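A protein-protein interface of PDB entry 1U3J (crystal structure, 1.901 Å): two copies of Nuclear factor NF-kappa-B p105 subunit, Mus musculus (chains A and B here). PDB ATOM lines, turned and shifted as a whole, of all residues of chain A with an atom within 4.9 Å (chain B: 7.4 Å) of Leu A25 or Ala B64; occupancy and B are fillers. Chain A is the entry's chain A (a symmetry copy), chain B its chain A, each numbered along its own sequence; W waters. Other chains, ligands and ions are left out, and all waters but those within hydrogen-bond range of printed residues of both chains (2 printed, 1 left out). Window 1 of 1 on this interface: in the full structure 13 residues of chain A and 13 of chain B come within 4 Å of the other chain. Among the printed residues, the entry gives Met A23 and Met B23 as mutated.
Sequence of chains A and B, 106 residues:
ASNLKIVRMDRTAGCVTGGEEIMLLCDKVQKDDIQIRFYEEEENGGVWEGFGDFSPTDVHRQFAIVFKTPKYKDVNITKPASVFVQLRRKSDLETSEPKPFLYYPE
O of Leu A25 is in hydrogen-bond range of N of Val A7 (2.8 Å).
O of Arg A8 lies within hydrogen-bond range of N of Leu A25.
The side-chain sulfur (SG) of Cys B26 sits at hydrogen-bond distance from the backbone NH (N) of Ala B64 (3.7 Å).
N of Ala A64 is in hydrogen-bond range of SG of Cys A26, at 3.7 Å.
The backbone carbonyl oxygen (O) of Asp B58 sits at hydrogen-bond distance from the backbone NH (N) of Val B66 (3.0 Å).
N of Cys A26 is in hydrogen-bond range of O of Phe A63, 3.0 Å away.
Met A23 touches its own counterpart, Met B23.
Met A23 touches Leu B25, and with the chains exchanged Leu A25 touches Met B23.
Leu A25 touches Ala B64, and with the chains exchanged Ala A64 touches Leu B25.
Phe A63 touches its own counterpart, Phe B63.
Of the 19 printed residues of chain B, 7 touch a printed residue of chain A.
Printed residues of chain B that touch a printed residue of chain A: Met B23, Leu B25, His B60, Arg B61, Phe B63, Ala B64 and Val B66.
Hydrophobic or aromatic side chains of chain B that line the printed part of chain A: Met B23, Leu B25, His B60, Phe B63, Ala B64 and Val B66.
Of the 11 printed residues of chain A, 7 touch a printed residue of chain B.
Hydrophobic or aromatic side chains of chain A within 4 Å of the printed part of chain B: Val A7, Met A23, Leu A25, Phe A63 and Ala A64.
Among the printed residues, 14 pairs touch across the chains.
Among the printed residues, no Asp or Glu carboxylate lies within 4 Å of a Lys or Arg side-chain nitrogen of the other chain.
Water W1 bridges OD1 of Asp A27 (2.5 Å) and NH1 of Arg B61 (2.7 Å).
Water W2 bridges the side-chain carboxylate (OD1) of Asp B58 and the guanidinium group (NH2) of Arg A8.
CE1 of His B60 touches CG2 of Val A7 (3.9 Å).
Arg A8 touches Met B23.
CG1 of Val B66 touches NE of Arg A8, at 3.96 Å.
Leu B25 touches Met A23 (CG to SD, 3.9 Å).
Met B23 touches Leu A25 (SD to CG, 3.9 Å).
His B60 touches Leu A25.
CB of Ala B64 touches CD2 of Leu A25, at 3.8 Å.
Leu A25 touches Val B66 (CD1 to CG2, 3.8 Å).
Phe A63 touches Phe B63 (CD2 to CD2, 3.7 Å).
CB of Ala A64 touches CD2 of Leu B25 (3.8 Å).
Leu A25 touches just these residues of chain B: Met B23 (3.9 Å), His B60 (3.9 Å), Ala B64 (3.8 Å) and Val B66 (3.8 Å).
Of chain A, only Leu A25 (3.8 Å) comes within 4 Å of Ala B64.
Printed residues of chain B within 4 Å of Met A23: Met B23 (3.8 Å) and Leu B25 (3.9 Å).
Printed residues of chain B within 4 Å of Arg A8: Met B23 (3.7 Å) and Val B66 (3.96 Å).
Of the printed residues of chain A, Arg B61 touches Phe A63 (3.3 Å).
Of the printed residues of chain B, Ala A64 touches Leu B25 (3.8 Å).
Lys A5 touches none of the printed residues of chain B.
Val B59 touches none of the printed residues of chain A.
The nearest printed residue of chain A that does not touch Ala B64 is Ala A64 (5.3 Å).
The nearest printed residue of chain A that does not touch Met B23 is Leu A24 (4.9 Å).
O of Cys A26 lies within hydrogen-bond range of NE2 of His B60, at 2.9 Å.
NE2 of His B60 is in hydrogen-bond range of O of Phe A63, at 2.8 Å.
The backbone carbonyl oxygen (O) of Met A23 lies close to the side-chain sulfur (SD) of Met B23 (3.8 Å).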
ATOM      1  N   LYS A   5      36.053 -36.892   9.107  1.00  0.00           N
ATOM      2  CA  LYS A   5      35.121 -36.184   9.930  1.00  0.00           C
ATOM      3  C   LYS A   5      33.712 -36.172   9.332  1.00  0.00           C
ATOM      4  O   LYS A   5      33.567 -35.894   8.151  1.00  0.00           O
ATOM      5  CB  LYS A   5      35.609 -34.756  10.157  1.00  0.00           C
ATOM      6  CG  LYS A   5      34.684 -33.976  11.080  1.00  0.00           C
ATOM      7  CD  LYS A   5      35.180 -32.541  11.295  1.00  0.00           C
ATOM      8  CE  LYS A   5      34.109 -31.712  12.032  1.00  0.00           C
ATOM      9  NZ  LYS A   5      34.511 -30.264  12.115  1.00  0.00           N
ATOM     10  N   ILE A   6      32.711 -36.529  10.152  1.00  0.00           N
ATOM     11  CA  ILE A   6      31.304 -36.383   9.776  1.00  0.00           C
ATOM     12  C   ILE A   6      30.917 -34.989  10.216  1.00  0.00           C
ATOM     13  O   ILE A   6      30.924 -34.681  11.390  1.00  0.00           O
ATOM     14  CB  ILE A   6      30.381 -37.411  10.443  1.00  0.00           C
ATOM     15  CG1 ILE A   6      30.783 -38.812  10.056  1.00  0.00           C
ATOM     16  CG2 ILE A   6      28.877 -37.104  10.061  1.00  0.00           C
ATOM     17  CD1 ILE A   6      30.165 -39.900  10.878  1.00  0.00           C
ATOM     18  N   VAL A   7      30.702 -34.107   9.246  1.00  0.00           N
ATOM     19  CA  VAL A   7      30.397 -32.716   9.531  1.00  0.00           C
ATOM     20  C   VAL A   7      28.939 -32.532   9.856  1.00  0.00           C
ATOM     21  O   VAL A   7      28.556 -31.794  10.784  1.00  0.00           O
ATOM     22  CB  VAL A   7      30.772 -31.843   8.296  1.00  0.00           C
ATOM     23  CG1 VAL A   7      30.185 -30.438   8.426  1.00  0.00           C
ATOM     24  CG2 VAL A   7      32.270 -31.783   8.161  1.00  0.00           C
ATOM     25  N   ARG A   8      28.096 -33.273   9.148  1.00  0.00           N
ATOM     26  CA  ARG A   8      26.671 -33.261   9.427  1.00  0.00           C
ATOM     27  C   ARG A   8      25.984 -34.430   8.786  1.00  0.00           C
ATOM     28  O   ARG A   8      26.393 -34.894   7.730  1.00  0.00           O
ATOM     29  CB  ARG A   8      26.037 -31.987   8.857  1.00  0.00           C
ATOM     30  CG  ARG A   8      25.114 -31.276   9.827  1.00  0.00           C
ATOM     31  CD  ARG A   8      23.701 -31.116   9.409  1.00  0.00           C
ATOM     32  NE  ARG A   8      23.221 -29.738   9.514  1.00  0.00           N
ATOM     33  CZ  ARG A   8      23.233 -28.991  10.615  1.00  0.00           C
ATOM     34  NH1 ARG A   8      23.705 -29.462  11.781  1.00  0.00           N
ATOM     35  NH2 ARG A   8      22.775 -27.740  10.552  1.00  0.00           N
ATOM     36  N   MET A  23      21.833 -38.413   3.893  1.00  0.00           N
ATOM     37  CA  MET A  23      22.864 -37.573   3.365  1.00  0.00           C
ATOM     38  C   MET A  23      23.784 -37.157   4.506  1.00  0.00           C
ATOM     39  O   MET A  23      23.322 -36.647   5.516  1.00  0.00           O
ATOM     40  CB  MET A  23      22.253 -36.325   2.797  1.00  0.00           C
ATOM     41  CG  MET A  23      22.701 -36.012   1.507  1.00  0.00           C
ATOM     42  SD  MET A  23      21.756 -34.665   0.733  1.00  0.00           S
ATOM     43  CE  MET A  23      20.881 -35.378  -0.497  1.00  0.00           C
ATOM     44  N   LEU A  24      25.052 -37.414   4.295  1.00  0.00           N
ATOM     45  CA  LEU A  24      26.130 -37.113   5.211  1.00  0.00           C
ATOM     46  C   LEU A  24      27.147 -36.222   4.510  1.00  0.00           C
ATOM     47  O   LEU A  24      27.548 -36.485   3.382  1.00  0.00           O
ATOM     48  CB  LEU A  24      26.720 -38.454   5.627  1.00  0.00           C
ATOM     49  CG  LEU A  24      27.905 -38.564   6.549  1.00  0.00           C
ATOM     50  CD1 LEU A  24      27.863 -39.945   7.190  1.00  0.00           C
ATOM     51  CD2 LEU A  24      29.210 -38.296   5.814  1.00  0.00           C
ATOM     52  N   LEU A  25      27.487 -35.123   5.153  1.00  0.00           N
ATOM     53  CA  LEU A  25      28.514 -34.208   4.729  1.00  0.00           C
ATOM     54  C   LEU A  25      29.777 -34.570   5.517  1.00  0.00           C
ATOM     55  O   LEU A  25      29.706 -34.781   6.733  1.00  0.00           O
ATOM     56  CB  LEU A  25      28.109 -32.775   5.078  1.00  0.00           C
ATOM     57  CG  LEU A  25      26.742 -32.335   4.537  1.00  0.00           C
ATOM     58  CD1 LEU A  25      26.540 -30.870   4.823  1.00  0.00           C
ATOM     59  CD2 LEU A  25      26.633 -32.685   3.031  1.00  0.00           C
ATOM     60  N   CYS A  26      30.905 -34.636   4.832  1.00  0.00           N
ATOM     61  CA  CYS A  26      32.166 -35.072   5.442  1.00  0.00           C
ATOM     62  C   CYS A  26      33.278 -34.220   4.900  1.00  0.00           C
ATOM     63  O   CYS A  26      33.153 -33.603   3.855  1.00  0.00           O
ATOM     64  CB  CYS A  26      32.450 -36.543   5.055  1.00  0.00           C
ATOM     65  SG  CYS A  26      32.338 -36.955   3.295  1.00  0.00           S
ATOM     66  N   ASP A  27      34.391 -34.203   5.592  1.00  0.00           N
ATOM     67  CA  ASP A  27      35.583 -33.642   5.000  1.00  0.00           C
ATOM     68  C   ASP A  27      36.099 -34.600   3.944  1.00  0.00           C
ATOM     69  O   ASP A  27      35.516 -35.654   3.747  1.00  0.00           O
ATOM     70  CB  ASP A  27      36.557 -33.310   6.105  1.00  0.00           C
ATOM     71  CG  ASP A  27      36.153 -32.036   6.819  1.00  0.00           C
ATOM     72  OD1 ASP A  27      35.416 -31.217   6.196  1.00  0.00           O
ATOM     73  OD2 ASP A  27      36.496 -31.769   7.973  1.00  0.00           O
ATOM     74  N   PHE A  63      33.053 -34.936  -0.743  1.00  0.00           N
ATOM     75  CA  PHE A  63      32.662 -34.142   0.421  1.00  0.00           C
ATOM     76  C   PHE A  63      31.271 -34.455   0.959  1.00  0.00           C
ATOM     77  O   PHE A  63      30.826 -33.822   1.898  1.00  0.00           O
ATOM     78  CB  PHE A  63      32.736 -32.651   0.076  1.00  0.00           C
ATOM     79  CG  PHE A  63      34.130 -32.102   0.064  1.00  0.00           C
ATOM     80  CD1 PHE A  63      34.844 -31.962   1.245  1.00  0.00           C
ATOM     81  CD2 PHE A  63      34.726 -31.699  -1.127  1.00  0.00           C
ATOM     82  CE1 PHE A  63      36.116 -31.423   1.255  1.00  0.00           C
ATOM     83  CE2 PHE A  63      36.030 -31.193  -1.127  1.00  0.00           C
ATOM     84  CZ  PHE A  63      36.718 -31.050   0.054  1.00  0.00           C
ATOM     85  N   ALA A  64      30.593 -35.433   0.360  1.00  0.00           N
ATOM     86  CA  ALA A  64      29.305 -35.910   0.865  1.00  0.00           C
ATOM     87  C   ALA A  64      29.051 -37.293   0.368  1.00  0.00           C
ATOM     88  O   ALA A  64      29.614 -37.719  -0.638  1.00  0.00           O
ATOM     89  CB  ALA A  64      28.113 -34.995   0.452  1.00  0.00           C
ATOM     90  N   MET B  23      19.139 -30.310   2.907  1.00  0.00           N
ATOM     91  CA  MET B  23      20.474 -30.487   2.423  1.00  0.00           C
ATOM     92  C   MET B  23      20.424 -30.658   0.910  1.00  0.00           C
ATOM     93  O   MET B  23      19.696 -31.501   0.409  1.00  0.00           O
ATOM     94  CB  MET B  23      21.056 -31.742   3.004  1.00  0.00           C
ATOM     95  CG  MET B  23      22.332 -31.572   3.557  1.00  0.00           C
ATOM     96  SD  MET B  23      22.903 -33.024   4.490  1.00  0.00           S
ATOM     97  CE  MET B  23      22.907 -32.555   6.093  1.00  0.00           C
ATOM     98  N   LEU B  24      21.195 -29.829   0.249  1.00  0.00           N
ATOM     99  CA  LEU B  24      21.338 -29.787  -1.189  1.00  0.00           C
ATOM    100  C   LEU B  24      22.805 -29.983  -1.550  1.00  0.00           C
ATOM    101  O   LEU B  24      23.689 -29.359  -0.971  1.00  0.00           O
ATOM    102  CB  LEU B  24      20.806 -28.431  -1.630  1.00  0.00           C
ATOM    103  CG  LEU B  24      20.826 -27.982  -3.067  1.00  0.00           C
ATOM    104  CD1 LEU B  24      19.753 -26.915  -3.231  1.00  0.00           C
ATOM    105  CD2 LEU B  24      22.208 -27.497  -3.480  1.00  0.00           C
ATOM    106  N   LEU B  25      23.057 -30.915  -2.446  1.00  0.00           N
ATOM    107  CA  LEU B  25      24.353 -31.179  -3.015  1.00  0.00           C
ATOM    108  C   LEU B  25      24.397 -30.450  -4.362  1.00  0.00           C
ATOM    109  O   LEU B  25      23.438 -30.528  -5.138  1.00  0.00           O
ATOM    110  CB  LEU B  25      24.516 -32.679  -3.261  1.00  0.00           C
ATOM    111  CG  LEU B  25      24.279 -33.569  -2.034  1.00  0.00           C
ATOM    112  CD1 LEU B  25      24.618 -34.996  -2.379  1.00  0.00           C
ATOM    113  CD2 LEU B  25      25.080 -33.025  -0.824  1.00  0.00           C
ATOM    114  N   CYS B  26      25.492 -29.761  -4.628  1.00  0.00           N
ATOM    115  CA  CYS B  26      25.624 -28.935  -5.833  1.00  0.00           C
ATOM    116  C   CYS B  26      27.021 -29.082  -6.364  1.00  0.00           C
ATOM    117  O   CYS B  26      27.930 -29.479  -5.654  1.00  0.00           O
ATOM    118  CB  CYS B  26      25.398 -27.447  -5.471  1.00  0.00           C
ATOM    119  SG  CYS B  26      26.343 -26.802  -4.067  1.00  0.00           S
ATOM    120  N   ASP B  27      27.211 -28.734  -7.613  1.00  0.00           N
ATOM    121  CA  ASP B  27      28.560 -28.582  -8.108  1.00  0.00           C
ATOM    122  C   ASP B  27      29.151 -27.314  -7.525  1.00  0.00           C
ATOM    123  O   ASP B  27      28.475 -26.613  -6.790  1.00  0.00           O
ATOM    124  CB  ASP B  27      28.529 -28.650  -9.616  1.00  0.00           C
ATOM    125  CG  ASP B  27      28.374 -30.080 -10.091  1.00  0.00           C
ATOM    126  OD1 ASP B  27      28.729 -31.007  -9.305  1.00  0.00           O
ATOM    127  OD2 ASP B  27      27.911 -30.381 -11.193  1.00  0.00           O
ATOM    128  N   LYS B  28      30.417 -27.000  -7.827  1.00  0.00           N
ATOM    129  CA  LYS B  28      31.116 -25.992  -7.037  1.00  0.00           C
ATOM    130  C   LYS B  28      30.467 -24.618  -7.057  1.00  0.00           C
ATOM    131  O   LYS B  28      30.285 -24.045  -8.126  1.00  0.00           O
ATOM    132  CB  LYS B  28      32.577 -25.847  -7.488  1.00  0.00           C
ATOM    133  CG  LYS B  28      33.479 -25.165  -6.486  1.00  0.00           C
ATOM    134  CD  LYS B  28      34.963 -25.347  -6.873  1.00  0.00           C
ATOM    135  CE  LYS B  28      35.888 -25.218  -5.682  1.00  0.00           C
ATOM    136  NZ  LYS B  28      37.323 -25.390  -6.084  1.00  0.00           N
ATOM    137  N   VAL B  29      30.225 -24.048  -5.873  1.00  0.00           N
ATOM    138  CA  VAL B  29      29.754 -22.682  -5.743  1.00  0.00           C
ATOM    139  C   VAL B  29      30.687 -21.851  -4.878  1.00  0.00           C
ATOM    140  O   VAL B  29      31.509 -22.398  -4.157  1.00  0.00           O
ATOM    141  CB  VAL B  29      28.348 -22.621  -5.123  1.00  0.00           C
ATOM    142  CG1 VAL B  29      27.384 -23.358  -5.993  1.00  0.00           C
ATOM    143  CG2 VAL B  29      28.330 -23.191  -3.685  1.00  0.00           C
ATOM    144  N   PHE B  54      20.047 -19.237   4.773  1.00  0.00           N
ATOM    145  CA  PHE B  54      21.338 -19.774   5.137  1.00  0.00           C
ATOM    146  C   PHE B  54      22.386 -18.671   5.075  1.00  0.00           C
ATOM    147  O   PHE B  54      22.192 -17.620   4.438  1.00  0.00           O
ATOM    148  CB  PHE B  54      21.751 -20.984   4.264  1.00  0.00           C
ATOM    149  CG  PHE B  54      22.088 -20.654   2.851  1.00  0.00           C
ATOM    150  CD1 PHE B  54      21.100 -20.492   1.902  1.00  0.00           C
ATOM    151  CD2 PHE B  54      23.418 -20.503   2.460  1.00  0.00           C
ATOM    152  CE1 PHE B  54      21.440 -20.209   0.565  1.00  0.00           C
ATOM    153  CE2 PHE B  54      23.756 -20.180   1.166  1.00  0.00           C
ATOM    154  CZ  PHE B  54      22.767 -20.035   0.213  1.00  0.00           C
ATOM    155  N   PRO B  56      26.918 -18.052   4.513  1.00  0.00           N
ATOM    156  CA  PRO B  56      28.099 -18.656   3.903  1.00  0.00           C
ATOM    157  C   PRO B  56      28.697 -19.805   4.698  1.00  0.00           C
ATOM    158  O   PRO B  56      29.171 -20.753   4.072  1.00  0.00           O
ATOM    159  CB  PRO B  56      29.080 -17.479   3.773  1.00  0.00           C
ATOM    160  CG  PRO B  56      28.126 -16.255   3.614  1.00  0.00           C
ATOM    161  CD  PRO B  56      27.038 -16.573   4.575  1.00  0.00           C
ATOM    162  N   THR B  57      28.619 -19.760   6.016  1.00  0.00           N
ATOM    163  CA  THR B  57      29.070 -20.897   6.828  1.00  0.00           C
ATOM    164  C   THR B  57      28.253 -22.184   6.672  1.00  0.00           C
ATOM    165  O   THR B  57      28.749 -23.244   7.013  1.00  0.00           O
ATOM    166  CB  THR B  57      29.158 -20.532   8.329  1.00  0.00           C
ATOM    167  OG1 THR B  57      27.916 -19.957   8.792  1.00  0.00           O
ATOM    168  CG2 THR B  57      30.211 -19.454   8.549  1.00  0.00           C
ATOM    169  N   ASP B  58      27.033 -22.095   6.166  1.00  0.00           N
ATOM    170  CA  ASP B  58      26.173 -23.280   5.924  1.00  0.00           C
ATOM    171  C   ASP B  58      26.442 -23.961   4.586  1.00  0.00           C
ATOM    172  O   ASP B  58      25.801 -24.975   4.227  1.00  0.00           O
ATOM    173  CB  ASP B  58      24.706 -22.872   5.978  1.00  0.00           C
ATOM    174  CG  ASP B  58      24.307 -22.313   7.309  1.00  0.00           C
ATOM    175  OD1 ASP B  58      24.745 -22.905   8.304  1.00  0.00           O
ATOM    176  OD2 ASP B  58      23.544 -21.327   7.459  1.00  0.00           O
ATOM    177  N   VAL B  59      27.362 -23.389   3.832  1.00  0.00           N
ATOM    178  CA  VAL B  59      27.839 -23.971   2.594  1.00  0.00           C
ATOM    179  C   VAL B  59      29.052 -24.819   2.954  1.00  0.00           C
ATOM    180  O   VAL B  59      30.017 -24.323   3.571  1.00  0.00           O
ATOM    181  CB  VAL B  59      28.240 -22.883   1.577  1.00  0.00           C
ATOM    182  CG1 VAL B  59      28.727 -23.531   0.298  1.00  0.00           C
ATOM    183  CG2 VAL B  59      27.050 -21.911   1.288  1.00  0.00           C
ATOM    184  N   HIS B  60      28.995 -26.088   2.571  1.00  0.00           N
ATOM    185  CA  HIS B  60      29.969 -27.079   2.972  1.00  0.00           C
ATOM    186  C   HIS B  60      30.956 -27.318   1.844  1.00  0.00           C
ATOM    187  O   HIS B  60      30.669 -28.009   0.852  1.00  0.00           O
ATOM    188  CB  HIS B  60      29.282 -28.395   3.372  1.00  0.00           C
ATOM    189  CG  HIS B  60      30.217 -29.553   3.515  1.00  0.00           C
ATOM    190  ND1 HIS B  60      31.129 -29.651   4.547  1.00  0.00           N
ATOM    191  CD2 HIS B  60      30.378 -30.669   2.758  1.00  0.00           C
ATOM    192  CE1 HIS B  60      31.795 -30.792   4.427  1.00  0.00           C
ATOM    193  NE2 HIS B  60      31.350 -31.433   3.358  1.00  0.00           N
ATOM    194  N   ARG B  61      32.137 -26.769   2.046  1.00  0.00           N
ATOM    195  CA  ARG B  61      33.305 -26.925   1.160  1.00  0.00           C
ATOM    196  C   ARG B  61      32.946 -26.688  -0.306  1.00  0.00           C
ATOM    197  O   ARG B  61      33.435 -27.396  -1.164  1.00  0.00           O
ATOM    198  CB  ARG B  61      33.969 -28.304   1.368  1.00  0.00           C
ATOM    199  CG  ARG B  61      34.484 -28.537   2.854  1.00  0.00           C
ATOM    200  CD  ARG B  61      35.392 -27.454   3.405  1.00  0.00           C
ATOM    201  NE  ARG B  61      36.406 -27.045   2.426  1.00  0.00           N
ATOM    202  CZ  ARG B  61      37.489 -27.761   2.101  1.00  0.00           C
ATOM    203  NH1 ARG B  61      37.749 -28.902   2.714  1.00  0.00           N
ATOM    204  NH2 ARG B  61      38.331 -27.310   1.168  1.00  0.00           N
ATOM    205  N   GLN B  62      32.040 -25.731  -0.550  1.00  0.00           N
ATOM    206  CA  GLN B  62      31.623 -25.341  -1.909  1.00  0.00           C
ATOM    207  C   GLN B  62      30.801 -26.379  -2.710  1.00  0.00           C
ATOM    208  O   GLN B  62      30.514 -26.165  -3.908  1.00  0.00           O
ATOM    209  CB  GLN B  62      32.858 -24.908  -2.724  1.00  0.00           C
ATOM    210  CG  GLN B  62      33.663 -23.837  -2.031  1.00  0.00           C
ATOM    211  CD  GLN B  62      34.854 -23.333  -2.839  1.00  0.00           C
ATOM    212  OE1 GLN B  62      34.769 -22.309  -3.496  1.00  0.00           O
ATOM    213  NE2 GLN B  62      35.965 -24.026  -2.741  1.00  0.00           N
ATOM    214  N   PHE B  63      30.396 -27.483  -2.068  1.00  0.00           N
ATOM    215  CA  PHE B  63      29.732 -28.573  -2.781  1.00  0.00           C
ATOM    216  C   PHE B  63      28.413 -29.020  -2.160  1.00  0.00           C
ATOM    217  O   PHE B  63      27.797 -29.950  -2.646  1.00  0.00           O
ATOM    218  CB  PHE B  63      30.672 -29.780  -2.869  1.00  0.00           C
ATOM    219  CG  PHE B  63      31.740 -29.638  -3.910  1.00  0.00           C
ATOM    220  CD1 PHE B  63      31.419 -29.667  -5.259  1.00  0.00           C
ATOM    221  CD2 PHE B  63      33.075 -29.499  -3.544  1.00  0.00           C
ATOM    222  CE1 PHE B  63      32.397 -29.575  -6.232  1.00  0.00           C
ATOM    223  CE2 PHE B  63      34.064 -29.362  -4.525  1.00  0.00           C
ATOM    224  CZ  PHE B  63      33.730 -29.406  -5.857  1.00  0.00           C
ATOM    225  N   ALA B  64      27.988 -28.352  -1.089  1.00  0.00           N
ATOM    226  CA  ALA B  64      26.679 -28.602  -0.484  1.00  0.00           C
ATOM    227  C   ALA B  64      26.252 -27.411   0.304  1.00  0.00           C
ATOM    228  O   ALA B  64      27.073 -26.595   0.718  1.00  0.00           O
ATOM    229  CB  ALA B  64      26.667 -29.855   0.443  1.00  0.00           C
ATOM    230  N   ILE B  65      24.946 -27.305   0.499  1.00  0.00           N
ATOM    231  CA  ILE B  65      24.332 -26.217   1.232  1.00  0.00           C
ATOM    232  C   ILE B  65      23.255 -26.762   2.138  1.00  0.00           C
ATOM    233  O   ILE B  65      22.334 -27.499   1.720  1.00  0.00           O
ATOM    234  CB  ILE B  65      23.737 -25.125   0.306  1.00  0.00           C
ATOM    235  CG1 ILE B  65      24.748 -24.652  -0.743  1.00  0.00           C
ATOM    236  CG2 ILE B  65      23.233 -23.935   1.169  1.00  0.00           C
ATOM    237  CD1 ILE B  65      24.159 -23.685  -1.774  1.00  0.00           C
ATOM    238  N   VAL B  66      23.328 -26.378   3.403  1.00  0.00           N
ATOM    239  CA  VAL B  66      22.234 -26.651   4.337  1.00  0.00           C
ATOM    240  C   VAL B  66      21.481 -25.353   4.576  1.00  0.00           C
ATOM    241  O   VAL B  66      22.072 -24.364   4.940  1.00  0.00           O
ATOM    242  CB  VAL B  66      22.794 -27.152   5.695  1.00  0.00           C
ATOM    243  CG1 VAL B  66      21.684 -27.599   6.559  1.00  0.00           C
ATOM    244  CG2 VAL B  66      23.837 -28.269   5.514  1.00  0.00           C
HETATM  245  O   HOH W   1      36.892 -29.450   5.250  1.00  0.00           O
HETATM  246  O   HOH W   2      24.735 -26.080   8.553  1.00  0.00           O
